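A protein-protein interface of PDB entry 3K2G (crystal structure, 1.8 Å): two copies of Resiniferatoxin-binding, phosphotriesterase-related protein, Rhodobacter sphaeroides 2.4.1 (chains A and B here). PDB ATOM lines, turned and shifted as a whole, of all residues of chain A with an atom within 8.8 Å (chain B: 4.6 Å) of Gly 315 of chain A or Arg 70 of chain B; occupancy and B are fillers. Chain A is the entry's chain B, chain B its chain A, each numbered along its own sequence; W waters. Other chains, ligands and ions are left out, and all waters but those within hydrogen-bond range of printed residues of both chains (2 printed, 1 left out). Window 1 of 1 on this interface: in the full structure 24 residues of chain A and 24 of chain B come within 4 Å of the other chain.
Of the 12 printed residues of chain B, 6 touch a printed residue of chain A. Hydrophobic or aromatic side chains of chain B that line the printed part of chain A: Ile 63 and Leu 66.
The backbone NH (N) of Arg 313 of chain A sits at hydrogen-bond distance from the side-chain carboxylate (OE2) of Glu 91 of chain A, 3.0 Å away. N of Phe 269 of chain B lies within hydrogen-bond range of O of Arg 70 of chain B (2.9 Å). O of Met 309 of chain A lies close to N of Gly 316 of chain A. The backbone NH (N) of Asn 317 of chain A sits at hydrogen-bond distance from the backbone carbonyl oxygen (O) of Met 310 of chain A (3.3 Å). OE2 of Glu 91 of chain A is in hydrogen-bond range of OG1 of Thr 312 of chain A (2.7 Å). N of Gly 316 of chain A sits at hydrogen-bond distance from O of Leu 311 of chain A (2.8 Å).
The side-chain amide nitrogen of Asn 317 of chain A lies close to the guanidinium group of Arg 70 of chain B. A ring nitrogen (NE2) of His 325 of chain A lies within hydrogen-bond range of the side-chain carboxylate (OE2) of Glu 68 of chain B (2.8 Å). The backbone NH (N) of Gly 315 of chain A lies close to the backbone carbonyl oxygen (O) of Ile 63 of chain B, 3.3 Å away. OG of Ser 67 of chain B lies within hydrogen-bond range of ND2 of Asn 317 of chain A (2.7 Å). O of Gly 315 of chain A sits at hydrogen-bond distance from NH2 of Arg 70 of chain B, 3.0 Å away.
Ile 63 of chain A touches its own counterpart, Ile 63 of chain B. Leu 66 of chain B touches its own counterpart, Leu 66 of chain A. Positions printed for both chains: 63, 66, 70, 268 and 309.
Water W2 lies within hydrogen-bond range of the side-chain amide oxygen of Gln 71 of chain B and the guanidinium group of Arg 329 of chain A. Water W1 lies within hydrogen-bond range of N of Ser 67 of chain B, O of Gly 316 of chain A, O of Thr 312 of chain A and N of Leu 66 of chain B.
Among the printed residues, merely in contact across the chains: Ile 63 of chain A with Ile 63 of chain B (3.7 Å), Leu 66 of chain A with Leu 66 of chain B (3.6 Å), Thr 312 of chain A with Ile 63 of chain B (3.6 Å), Arg 313 of chain A with Ile 63 of chain B (3.6 Å), Tyr 314 of chain A with Ile 63 of chain B (3.4 Å), Gly 316 of chain A with Ser 67 of chain B (3.0 Å), Gly 316 of chain A with Arg 70 of chain B (3.98 Å), Phe 321 of chain A with Gln 71 of chain B (3.7 Å) and His 325 of chain A with Gln 71 of chain B (3.6 Å).
Ile 61 of chain A touches none of the printed residues of chain B. Of the printed residues of chain B, Ile 63 of chain A touches Ile 63. Met 310 of chain A touches none of the printed residues of chain B. Of the printed residues of chain B, Arg 313 of chain A touches Ile 63. Gly 315 of chain A touches just these residues of chain B: Ile 63 and Arg 70. Printed residues of chain B within 4 Å of Asn 317 of chain A: Ser 67 (2.7 Å) and Arg 70 (3.1 Å). Ser 67 of chain B touches just these residues of chain A: Gly 316 and Asn 317. Of the printed residues of chain A, Glu 68 of chain B touches His 325 (2.8 Å). Printed residues of chain A within 4 Å of Arg 70 of chain B: Gly 315 (3.0 Å), Gly 316 (3.98 Å) and Asn 317 (3.1 Å). Of chain A, only Phe 321 and His 325 come within 4 Å of Gln 71 of chain B. The nearest printed residue of chain A that does not touch Arg 70 of chain B is Arg 70 of chain A (5.2 Å). The nearest printed residue of chain B that does not touch Ile 63 of chain A is Leu 66 of chain B (4.1 Å).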
ATOM      1  N   ILE A  61      31.328 -16.804  22.882  1.00  0.00           N
ATOM      2  CA  ILE A  61      31.441 -17.119  21.465  1.00  0.00           C
ATOM      3  C   ILE A  61      31.756 -15.852  20.679  1.00  0.00           C
ATOM      4  O   ILE A  61      31.025 -14.864  20.755  1.00  0.00           O
ATOM      5  CB  ILE A  61      30.142 -17.740  20.900  1.00  0.00           C
ATOM      6  CG1 ILE A  61      29.848 -19.072  21.596  1.00  0.00           C
ATOM      7  CG2 ILE A  61      30.287 -17.964  19.401  1.00  0.00           C
ATOM      8  CD1 ILE A  61      28.486 -19.641  21.260  1.00  0.00           C
ATOM      9  N   SER A  62      32.860 -15.883  19.938  1.00  0.00           N
ATOM     10  CA  SER A  62      33.269 -14.753  19.111  1.00  0.00           C
ATOM     11  C   SER A  62      33.787 -15.310  17.789  1.00  0.00           C
ATOM     12  O   SER A  62      34.300 -16.428  17.740  1.00  0.00           O
ATOM     13  CB  SER A  62      34.378 -13.943  19.793  1.00  0.00           C
ATOM     14  OG  SER A  62      35.580 -14.691  19.877  1.00  0.00           O
ATOM     15  N   ILE A  63      33.660 -14.523  16.725  1.00  0.00           N
ATOM     16  CA  ILE A  63      34.096 -14.938  15.394  1.00  0.00           C
ATOM     17  C   ILE A  63      35.524 -15.490  15.360  1.00  0.00           C
ATOM     18  O   ILE A  63      35.839 -16.381  14.561  1.00  0.00           O
ATOM     19  CB  ILE A  63      33.970 -13.756  14.386  1.00  0.00           C
ATOM     20  CG1 ILE A  63      34.250 -14.240  12.962  1.00  0.00           C
ATOM     21  CG2 ILE A  63      34.936 -12.627  14.754  1.00  0.00           C
ATOM     22  CD1 ILE A  63      33.980 -13.183  11.911  1.00  0.00           C
ATOM     23  N   LEU A  66      35.613 -19.533  16.232  1.00  0.00           N
ATOM     24  CA  LEU A  66      34.659 -20.465  15.646  1.00  0.00           C
ATOM     25  C   LEU A  66      35.284 -21.746  15.098  1.00  0.00           C
ATOM     26  O   LEU A  66      34.695 -22.825  15.214  1.00  0.00           O
ATOM     27  CB  LEU A  66      33.845 -19.777  14.551  1.00  0.00           C
ATOM     28  CG  LEU A  66      32.957 -18.631  15.054  1.00  0.00           C
ATOM     29  CD1 LEU A  66      32.176 -18.056  13.896  1.00  0.00           C
ATOM     30  CD2 LEU A  66      32.018 -19.135  16.143  1.00  0.00           C
ATOM     31  N   ARG A  70      34.151 -25.480  16.314  1.00  0.00           N
ATOM     32  CA  ARG A  70      33.618 -26.491  15.407  1.00  0.00           C
ATOM     33  C   ARG A  70      34.280 -27.867  15.599  1.00  0.00           C
ATOM     34  O   ARG A  70      33.709 -28.892  15.219  1.00  0.00           O
ATOM     35  CB  ARG A  70      33.770 -26.041  13.942  1.00  0.00           C
ATOM     36  CG  ARG A  70      32.884 -24.850  13.550  1.00  0.00           C
ATOM     37  CD  ARG A  70      32.877 -24.630  12.038  1.00  0.00           C
ATOM     38  NE  ARG A  70      34.158 -24.163  11.506  1.00  0.00           N
ATOM     39  CZ  ARG A  70      34.513 -22.883  11.400  1.00  0.00           C
ATOM     40  NH1 ARG A  70      33.684 -21.922  11.789  1.00  0.00           N
ATOM     41  NH2 ARG A  70      35.698 -22.560  10.896  1.00  0.00           N
ATOM     42  N   GLU A  91      15.726 -15.269  15.146  1.00  0.00           N
ATOM     43  CA  GLU A  91      16.219 -16.389  14.354  1.00  0.00           C
ATOM     44  C   GLU A  91      15.066 -17.181  13.741  1.00  0.00           C
ATOM     45  O   GLU A  91      15.169 -17.655  12.613  1.00  0.00           O
ATOM     46  CB  GLU A  91      17.080 -17.298  15.227  1.00  0.00           C
ATOM     47  CG  GLU A  91      18.423 -16.689  15.649  1.00  0.00           C
ATOM     48  CD  GLU A  91      19.471 -16.726  14.540  1.00  0.00           C
ATOM     49  OE1 GLU A  91      19.444 -17.671  13.719  1.00  0.00           O
ATOM     50  OE2 GLU A  91      20.335 -15.825  14.497  1.00  0.00           O
ATOM     51  N   GLY A 265      23.118 -29.491   7.919  1.00  0.00           N
ATOM     52  CA  GLY A 265      23.877 -28.282   8.180  1.00  0.00           C
ATOM     53  C   GLY A 265      24.891 -28.435   9.296  1.00  0.00           C
ATOM     54  O   GLY A 265      25.827 -27.633   9.393  1.00  0.00           O
ATOM     55  N   MET A 266      24.707 -29.454  10.138  1.00  0.00           N
ATOM     56  CA  MET A 266      25.620 -29.711  11.257  1.00  0.00           C
ATOM     57  C   MET A 266      26.838 -30.476  10.774  1.00  0.00           C
ATOM     58  O   MET A 266      26.739 -31.634  10.366  1.00  0.00           O
ATOM     59  CB  MET A 266      24.927 -30.518  12.362  1.00  0.00           C
ATOM     60  CG  MET A 266      25.829 -30.999  13.526  1.00  0.00           C
ATOM     61  SD  MET A 266      24.733 -31.850  14.848  1.00  0.00           S
ATOM     62  CE  MET A 266      25.698 -33.511  15.331  1.00  0.00           C
ATOM     63  N   ASP A 267      27.992 -29.828  10.840  1.00  0.00           N
ATOM     64  CA  ASP A 267      29.225 -30.446  10.387  1.00  0.00           C
ATOM     65  C   ASP A 267      30.323 -30.437  11.445  1.00  0.00           C
ATOM     66  O   ASP A 267      31.508 -30.418  11.106  1.00  0.00           O
ATOM     67  CB  ASP A 267      29.713 -29.723   9.129  1.00  0.00           C
ATOM     68  CG  ASP A 267      30.068 -28.267   9.391  1.00  0.00           C
ATOM     69  OD1 ASP A 267      29.450 -27.641  10.281  1.00  0.00           O
ATOM     70  OD2 ASP A 267      30.963 -27.743   8.693  1.00  0.00           O
ATOM     71  N   PHE A 268      29.936 -30.462  12.717  1.00  0.00           N
ATOM     72  CA  PHE A 268      30.913 -30.443  13.801  1.00  0.00           C
ATOM     73  C   PHE A 268      31.563 -31.799  14.046  1.00  0.00           C
ATOM     74  O   PHE A 268      31.061 -32.837  13.608  1.00  0.00           O
ATOM     75  CB  PHE A 268      30.265 -30.011  15.122  1.00  0.00           C
ATOM     76  CG  PHE A 268      29.346 -28.831  15.005  1.00  0.00           C
ATOM     77  CD1 PHE A 268      29.687 -27.733  14.221  1.00  0.00           C
ATOM     78  CD2 PHE A 268      28.153 -28.800  15.721  1.00  0.00           C
ATOM     79  CE1 PHE A 268      28.846 -26.615  14.151  1.00  0.00           C
ATOM     80  CE2 PHE A 268      27.308 -27.689  15.661  1.00  0.00           C
ATOM     81  CZ  PHE A 268      27.656 -26.597  14.877  1.00  0.00           C
ATOM     82  N   LYS A 308      24.155 -22.309  20.835  1.00  0.00           N
ATOM     83  CA  LYS A 308      24.260 -20.966  20.277  1.00  0.00           C
ATOM     84  C   LYS A 308      24.978 -20.867  18.934  1.00  0.00           C
ATOM     85  O   LYS A 308      24.535 -20.132  18.047  1.00  0.00           O
ATOM     86  CB  LYS A 308      24.961 -20.020  21.262  1.00  0.00           C
ATOM     87  CG  LYS A 308      24.182 -19.707  22.532  1.00  0.00           C
ATOM     88  CD  LYS A 308      24.738 -18.453  23.202  1.00  0.00           C
ATOM     89  CE  LYS A 308      23.986 -18.105  24.492  1.00  0.00           C
ATOM     90  NZ  LYS A 308      24.244 -19.102  25.569  1.00  0.00           N
ATOM     91  N   MET A 309      26.077 -21.602  18.776  1.00  0.00           N
ATOM     92  CA  MET A 309      26.844 -21.506  17.537  1.00  0.00           C
ATOM     93  C   MET A 309      26.112 -21.979  16.292  1.00  0.00           C
ATOM     94  O   MET A 309      26.607 -21.813  15.184  1.00  0.00           O
ATOM     95  CB  MET A 309      28.201 -22.224  17.663  1.00  0.00           C
ATOM     96  CG  MET A 309      28.168 -23.729  17.686  1.00  0.00           C
ATOM     97  SD  MET A 309      29.996 -24.416  17.902  1.00  0.00           S
ATOM     98  CE  MET A 309      30.644 -24.230  16.041  1.00  0.00           C
ATOM     99  N   MET A 310      24.920 -22.545  16.458  1.00  0.00           N
ATOM    100  CA  MET A 310      24.167 -22.994  15.298  1.00  0.00           C
ATOM    101  C   MET A 310      23.200 -21.911  14.828  1.00  0.00           C
ATOM    102  O   MET A 310      22.505 -22.083  13.832  1.00  0.00           O
ATOM    103  CB  MET A 310      23.421 -24.287  15.615  1.00  0.00           C
ATOM    104  CG  MET A 310      24.342 -25.500  15.794  1.00  0.00           C
ATOM    105  SD  MET A 310      23.408 -27.127  16.265  1.00  0.00           S
ATOM    106  CE  MET A 310      22.570 -27.491  14.525  1.00  0.00           C
ATOM    107  N   LEU A 311      23.166 -20.797  15.553  1.00  0.00           N
ATOM    108  CA  LEU A 311      22.307 -19.668  15.191  1.00  0.00           C
ATOM    109  C   LEU A 311      23.118 -18.749  14.275  1.00  0.00           C
ATOM    110  O   LEU A 311      24.336 -18.637  14.436  1.00  0.00           O
ATOM    111  CB  LEU A 311      21.882 -18.903  16.444  1.00  0.00           C
ATOM    112  CG  LEU A 311      21.066 -19.703  17.461  1.00  0.00           C
ATOM    113  CD1 LEU A 311      20.859 -18.868  18.717  1.00  0.00           C
ATOM    114  CD2 LEU A 311      19.730 -20.104  16.849  1.00  0.00           C
ATOM    115  N   THR A 312      22.452 -18.088  13.331  1.00  0.00           N
ATOM    116  CA  THR A 312      23.156 -17.217  12.395  1.00  0.00           C
ATOM    117  C   THR A 312      23.888 -16.085  13.129  1.00  0.00           C
ATOM    118  O   THR A 312      24.977 -15.662  12.724  1.00  0.00           O
ATOM    119  CB  THR A 312      22.188 -16.632  11.337  1.00  0.00           C
ATOM    120  OG1 THR A 312      21.332 -15.656  11.944  1.00  0.00           O
ATOM    121  CG2 THR A 312      21.326 -17.745  10.748  1.00  0.00           C
ATOM    122  N   ARG A 313      23.293 -15.616  14.220  1.00  0.00           N
ATOM    123  CA  ARG A 313      23.896 -14.560  15.026  1.00  0.00           C
ATOM    124  C   ARG A 313      25.312 -14.930  15.465  1.00  0.00           C
ATOM    125  O   ARG A 313      26.158 -14.055  15.662  1.00  0.00           O
ATOM    126  CB  ARG A 313      23.026 -14.299  16.256  1.00  0.00           C
ATOM    127  CG  ARG A 313      23.783 -13.874  17.504  1.00  0.00           C
ATOM    128  CD  ARG A 313      24.102 -12.401  17.511  1.00  0.00           C
ATOM    129  NE  ARG A 313      24.776 -12.001  18.749  1.00  0.00           N
ATOM    130  CZ  ARG A 313      26.094 -11.924  18.895  1.00  0.00           C
ATOM    131  NH1 ARG A 313      26.894 -12.221  17.877  1.00  0.00           N
ATOM    132  NH2 ARG A 313      26.612 -11.535  20.054  1.00  0.00           N
ATOM    133  N   TYR A 314      25.573 -16.224  15.622  1.00  0.00           N
ATOM    134  CA  TYR A 314      26.893 -16.676  16.048  1.00  0.00           C
ATOM    135  C   TYR A 314      27.687 -17.361  14.943  1.00  0.00           C
ATOM    136  O   TYR A 314      28.595 -18.146  15.226  1.00  0.00           O
ATOM    137  CB  TYR A 314      26.771 -17.616  17.245  1.00  0.00           C
ATOM    138  CG  TYR A 314      26.282 -16.926  18.491  1.00  0.00           C
ATOM    139  CD1 TYR A 314      27.083 -15.994  19.152  1.00  0.00           C
ATOM    140  CD2 TYR A 314      25.007 -17.179  18.995  1.00  0.00           C
ATOM    141  CE1 TYR A 314      26.622 -15.330  20.287  1.00  0.00           C
ATOM    142  CE2 TYR A 314      24.539 -16.522  20.126  1.00  0.00           C
ATOM    143  CZ  TYR A 314      25.349 -15.599  20.769  1.00  0.00           C
ATOM    144  OH  TYR A 314      24.885 -14.955  21.894  1.00  0.00           O
ATOM    145  N   GLY A 315      27.348 -17.055  13.695  1.00  0.00           N
ATOM    146  CA  GLY A 315      28.054 -17.637  12.569  1.00  0.00           C
ATOM    147  C   GLY A 315      27.504 -18.965  12.081  1.00  0.00           C
ATOM    148  O   GLY A 315      28.076 -19.585  11.175  1.00  0.00           O
ATOM    149  N   GLY A 316      26.393 -19.395  12.674  1.00  0.00           N
ATOM    150  CA  GLY A 316      25.782 -20.660  12.296  1.00  0.00           C
ATOM    151  C   GLY A 316      24.758 -20.565  11.181  1.00  0.00           C
ATOM    152  O   GLY A 316      24.584 -19.508  10.584  1.00  0.00           O
ATOM    153  N   ASN A 317      24.063 -21.673  10.923  1.00  0.00           N
ATOM    154  CA  ASN A 317      23.073 -21.752   9.847  1.00  0.00           C
ATOM    155  C   ASN A 317      21.655 -21.276  10.184  1.00  0.00           C
ATOM    156  O   ASN A 317      20.893 -20.922   9.288  1.00  0.00           O
ATOM    157  CB  ASN A 317      23.018 -23.190   9.324  1.00  0.00           C
ATOM    158  CG  ASN A 317      24.357 -23.656   8.766  1.00  0.00           C
ATOM    159  OD1 ASN A 317      24.730 -24.821   8.899  1.00  0.00           O
ATOM    160  ND2 ASN A 317      25.074 -22.749   8.129  1.00  0.00           N
ATOM    161  N   GLY A 318      21.302 -21.277  11.464  1.00  0.00           N
ATOM    162  CA  GLY A 318      19.974 -20.831  11.856  1.00  0.00           C
ATOM    163  C   GLY A 318      18.876 -21.840  11.567  1.00  0.00           C
ATOM    164  O   GLY A 318      19.151 -23.029  11.390  1.00  0.00           O
ATOM    165  N   PHE A 321      18.027 -22.620   7.100  1.00  0.00           N
ATOM    166  CA  PHE A 321      19.020 -23.282   6.263  1.00  0.00           C
ATOM    167  C   PHE A 321      18.457 -24.443   5.437  1.00  0.00           C
ATOM    168  O   PHE A 321      18.698 -24.536   4.238  1.00  0.00           O
ATOM    169  CB  PHE A 321      20.175 -23.770   7.143  1.00  0.00           C
ATOM    170  CG  PHE A 321      21.331 -24.327   6.370  1.00  0.00           C
ATOM    171  CD1 PHE A 321      22.241 -23.477   5.745  1.00  0.00           C
ATOM    172  CD2 PHE A 321      21.505 -25.703   6.253  1.00  0.00           C
ATOM    173  CE1 PHE A 321      23.309 -23.990   5.015  1.00  0.00           C
ATOM    174  CE2 PHE A 321      22.565 -26.227   5.525  1.00  0.00           C
ATOM    175  CZ  PHE A 321      23.472 -25.367   4.906  1.00  0.00           C
ATOM    176  N   HIS A 325      18.826 -23.543   1.703  1.00  0.00           N
ATOM    177  CA  HIS A 325      19.999 -24.149   1.105  1.00  0.00           C
ATOM    178  C   HIS A 325      19.970 -25.652   0.859  1.00  0.00           C
ATOM    179  O   HIS A 325      20.447 -26.107  -0.177  1.00  0.00           O
ATOM    180  CB  HIS A 325      21.220 -23.755   1.939  1.00  0.00           C
ATOM    181  CG  HIS A 325      21.439 -22.273   2.005  1.00  0.00           C
ATOM    182  ND1 HIS A 325      21.927 -21.542   0.943  1.00  0.00           N
ATOM    183  CD2 HIS A 325      21.208 -21.380   2.996  1.00  0.00           C
ATOM    184  CE1 HIS A 325      21.990 -20.266   1.276  1.00  0.00           C
ATOM    185  NE2 HIS A 325      21.559 -20.140   2.516  1.00  0.00           N
ATOM    186  N   ARG A 329      19.919 -28.170  -2.735  1.00  0.00           N
ATOM    187  CA  ARG A 329      20.942 -29.213  -2.851  1.00  0.00           C
ATOM    188  C   ARG A 329      20.269 -30.534  -3.246  1.00  0.00           C
ATOM    189  O   ARG A 329      20.776 -31.268  -4.091  1.00  0.00           O
ATOM    190  CB  ARG A 329      21.683 -29.386  -1.518  1.00  0.00           C
ATOM    191  CG  ARG A 329      22.820 -30.410  -1.535  1.00  0.00           C
ATOM    192  CD  ARG A 329      23.419 -30.594  -0.140  1.00  0.00           C
ATOM    193  NE  ARG A 329      24.089 -29.386   0.346  1.00  0.00           N
ATOM    194  CZ  ARG A 329      25.296 -28.983  -0.048  1.00  0.00           C
ATOM    195  NH1 ARG A 329      25.987 -29.689  -0.935  1.00  0.00           N
ATOM    196  NH2 ARG A 329      25.818 -27.864   0.445  1.00  0.00           N
ATOM    197  N   ILE B  63      30.398 -11.820  11.910  1.00  0.00           N
ATOM    198  CA  ILE B  63      29.938 -13.126  12.364  1.00  0.00           C
ATOM    199  C   ILE B  63      28.529 -13.530  11.925  1.00  0.00           C
ATOM    200  O   ILE B  63      28.291 -14.697  11.612  1.00  0.00           O
ATOM    201  CB  ILE B  63      30.037 -13.232  13.907  1.00  0.00           C
ATOM    202  CG1 ILE B  63      29.707 -14.655  14.363  1.00  0.00           C
ATOM    203  CG2 ILE B  63      29.099 -12.216  14.565  1.00  0.00           C
ATOM    204  CD1 ILE B  63      30.110 -14.945  15.802  1.00  0.00           C
ATOM    205  N   LEU B  66      28.258 -15.174   8.140  1.00  0.00           N
ATOM    206  CA  LEU B  66      29.137 -16.263   7.751  1.00  0.00           C
ATOM    207  C   LEU B  66      28.439 -17.447   7.090  1.00  0.00           C
ATOM    208  O   LEU B  66      28.982 -18.035   6.155  1.00  0.00           O
ATOM    209  CB  LEU B  66      29.933 -16.754   8.955  1.00  0.00           C
ATOM    210  CG  LEU B  66      30.929 -15.756   9.548  1.00  0.00           C
ATOM    211  CD1 LEU B  66      31.690 -16.439  10.664  1.00  0.00           C
ATOM    212  CD2 LEU B  66      31.899 -15.261   8.471  1.00  0.00           C
ATOM    213  N   SER B  67      27.248 -17.808   7.562  1.00  0.00           N
ATOM    214  CA  SER B  67      26.553 -18.945   6.959  1.00  0.00           C
ATOM    215  C   SER B  67      26.334 -18.681   5.480  1.00  0.00           C
ATOM    216  O   SER B  67      26.675 -19.506   4.631  1.00  0.00           O
ATOM    217  CB  SER B  67      25.200 -19.194   7.618  1.00  0.00           C
ATOM    218  OG  SER B  67      24.579 -20.328   7.028  1.00  0.00           O
ATOM    219  N   GLU B  68      25.767 -17.521   5.181  1.00  0.00           N
ATOM    220  CA  GLU B  68      25.503 -17.143   3.805  1.00  0.00           C
ATOM    221  C   GLU B  68      26.769 -17.096   2.953  1.00  0.00           C
ATOM    222  O   GLU B  68      26.761 -17.547   1.807  1.00  0.00           O
ATOM    223  CB  GLU B  68      24.793 -15.788   3.757  1.00  0.00           C
ATOM    224  CG  GLU B  68      23.325 -15.855   4.144  1.00  0.00           C
ATOM    225  CD  GLU B  68      22.559 -16.870   3.304  1.00  0.00           C
ATOM    226  OE1 GLU B  68      22.625 -16.779   2.056  1.00  0.00           O
ATOM    227  OE2 GLU B  68      21.900 -17.756   3.893  1.00  0.00           O
ATOM    228  N   LEU B  69      27.854 -16.555   3.505  1.00  0.00           N
ATOM    229  CA  LEU B  69      29.103 -16.467   2.751  1.00  0.00           C
ATOM    230  C   LEU B  69      29.634 -17.853   2.407  1.00  0.00           C
ATOM    231  O   LEU B  69      30.192 -18.059   1.330  1.00  0.00           O
ATOM    232  CB  LEU B  69      30.162 -15.674   3.535  1.00  0.00           C
ATOM    233  CG  LEU B  69      29.751 -14.233   3.855  1.00  0.00           C
ATOM    234  CD1 LEU B  69      30.892 -13.488   4.553  1.00  0.00           C
ATOM    235  CD2 LEU B  69      29.373 -13.530   2.558  1.00  0.00           C
ATOM    236  N   ARG B  70      29.456 -18.802   3.318  1.00  0.00           N
ATOM    237  CA  ARG B  70      29.917 -20.164   3.079  1.00  0.00           C
ATOM    238  C   ARG B  70      29.183 -20.806   1.894  1.00  0.00           C
ATOM    239  O   ARG B  70      29.670 -21.768   1.296  1.00  0.00           O
ATOM    240  CB  ARG B  70      29.733 -21.024   4.337  1.00  0.00           C
ATOM    241  CG  ARG B  70      30.704 -20.709   5.483  1.00  0.00           C
ATOM    242  CD  ARG B  70      30.709 -21.815   6.541  1.00  0.00           C
ATOM    243  NE  ARG B  70      29.422 -21.988   7.224  1.00  0.00           N
ATOM    244  CZ  ARG B  70      29.009 -21.258   8.260  1.00  0.00           C
ATOM    245  NH1 ARG B  70      29.781 -20.294   8.744  1.00  0.00           N
ATOM    246  NH2 ARG B  70      27.828 -21.503   8.823  1.00  0.00           N
ATOM    247  N   GLN B  71      28.018 -20.264   1.553  1.00  0.00           N
ATOM    248  CA  GLN B  71      27.229 -20.791   0.443  1.00  0.00           C
ATOM    249  C   GLN B  71      27.477 -20.021  -0.856  1.00  0.00           C
ATOM    250  O   GLN B  71      26.949 -20.380  -1.911  1.00  0.00           O
ATOM    251  CB  GLN B  71      25.736 -20.735   0.782  1.00  0.00           C
ATOM    252  CG  GLN B  71      25.363 -21.307   2.150  1.00  0.00           C
ATOM    253  CD  GLN B  71      25.937 -22.685   2.394  1.00  0.00           C
ATOM    254  OE1 GLN B  71      25.822 -23.582   1.556  1.00  0.00           O
ATOM    255  NE2 GLN B  71      26.556 -22.867   3.551  1.00  0.00           N
ATOM    256  N   ASP B  72      28.285 -18.970  -0.776  1.00  0.00           N
ATOM    257  CA  ASP B  72      28.594 -18.136  -1.936  1.00  0.00           C
ATOM    258  C   ASP B  72      29.736 -17.180  -1.573  1.00  0.00           C
ATOM    259  O   ASP B  72      29.548 -15.966  -1.516  1.00  0.00           O
ATOM    260  CB  ASP B  72      27.349 -17.337  -2.337  1.00  0.00           C
ATOM    261  CG  ASP B  72      27.521 -16.599  -3.657  1.00  0.00           C
ATOM    262  OD1 ASP B  72      28.525 -16.856  -4.357  1.00  0.00           O
ATOM    263  OD2 ASP B  72      26.646 -15.774  -4.000  1.00  0.00           O
ATOM    264  N   PRO B  73      30.941 -17.727  -1.341  1.00  0.00           N
ATOM    265  CA  PRO B  73      32.152 -16.983  -0.973  1.00  0.00           C
ATOM    266  C   PRO B  73      32.456 -15.708  -1.765  1.00  0.00           C
ATOM    267  O   PRO B  73      32.819 -14.687  -1.178  1.00  0.00           O
ATOM    268  CB  PRO B  73      33.255 -18.029  -1.126  1.00  0.00           C
ATOM    269  CG  PRO B  73      32.549 -19.311  -0.788  1.00  0.00           C
ATOM    270  CD  PRO B  73      31.255 -19.153  -1.553  1.00  0.00           C
ATOM    271  N   PHE B 268      33.219 -24.947   1.702  1.00  0.00           N
ATOM    272  CA  PHE B 268      32.252 -24.044   1.082  1.00  0.00           C
ATOM    273  C   PHE B 268      31.520 -24.634  -0.112  1.00  0.00           C
ATOM    274  O   PHE B 268      31.960 -25.612  -0.714  1.00  0.00           O
ATOM    275  CB  PHE B 268      32.931 -22.759   0.594  1.00  0.00           C
ATOM    276  CG  PHE B 268      33.919 -22.177   1.557  1.00  0.00           C
ATOM    277  CD1 PHE B 268      33.616 -22.070   2.912  1.00  0.00           C
ATOM    278  CD2 PHE B 268      35.154 -21.720   1.105  1.00  0.00           C
ATOM    279  CE1 PHE B 268      34.528 -21.505   3.804  1.00  0.00           C
ATOM    280  CE2 PHE B 268      36.072 -21.154   1.987  1.00  0.00           C
ATOM    281  CZ  PHE B 268      35.762 -21.049   3.338  1.00  0.00           C
ATOM    282  N   PHE B 269      30.384 -24.028  -0.440  1.00  0.00           N
ATOM    283  CA  PHE B 269      29.630 -24.426  -1.620  1.00  0.00           C
ATOM    284  C   PHE B 269      29.848 -23.241  -2.543  1.00  0.00           C
ATOM    285  O   PHE B 269      29.471 -22.114  -2.213  1.00  0.00           O
ATOM    286  CB  PHE B 269      28.132 -24.564  -1.351  1.00  0.00           C
ATOM    287  CG  PHE B 269      27.319 -24.783  -2.605  1.00  0.00           C
ATOM    288  CD1 PHE B 269      27.435 -25.973  -3.326  1.00  0.00           C
ATOM    289  CD2 PHE B 269      26.483 -23.782  -3.094  1.00  0.00           C
ATOM    290  CE1 PHE B 269      26.732 -26.163  -4.518  1.00  0.00           C
ATOM    291  CE2 PHE B 269      25.774 -23.958  -4.286  1.00  0.00           C
ATOM    292  CZ  PHE B 269      25.899 -25.152  -5.001  1.00  0.00           C
ATOM    293  N   MET B 309      37.689 -14.925   4.738  1.00  0.00           N
ATOM    294  CA  MET B 309      36.910 -15.788   5.626  1.00  0.00           C
ATOM    295  C   MET B 309      37.626 -17.082   5.993  1.00  0.00           C
ATOM    296  O   MET B 309      37.157 -17.836   6.850  1.00  0.00           O
ATOM    297  CB  MET B 309      35.535 -16.114   5.024  1.00  0.00           C
ATOM    298  CG  MET B 309      35.555 -17.069   3.849  1.00  0.00           C
ATOM    299  SD  MET B 309      33.741 -17.253   3.111  1.00  0.00           S
ATOM    300  CE  MET B 309      32.898 -18.147   4.668  1.00  0.00           C
HETATM  301  O   HOH W   1      25.892 -16.872   9.958  1.00  0.00           O
HETATM  302  O   HOH W   2      24.251 -25.502   1.129  1.00  0.00           O
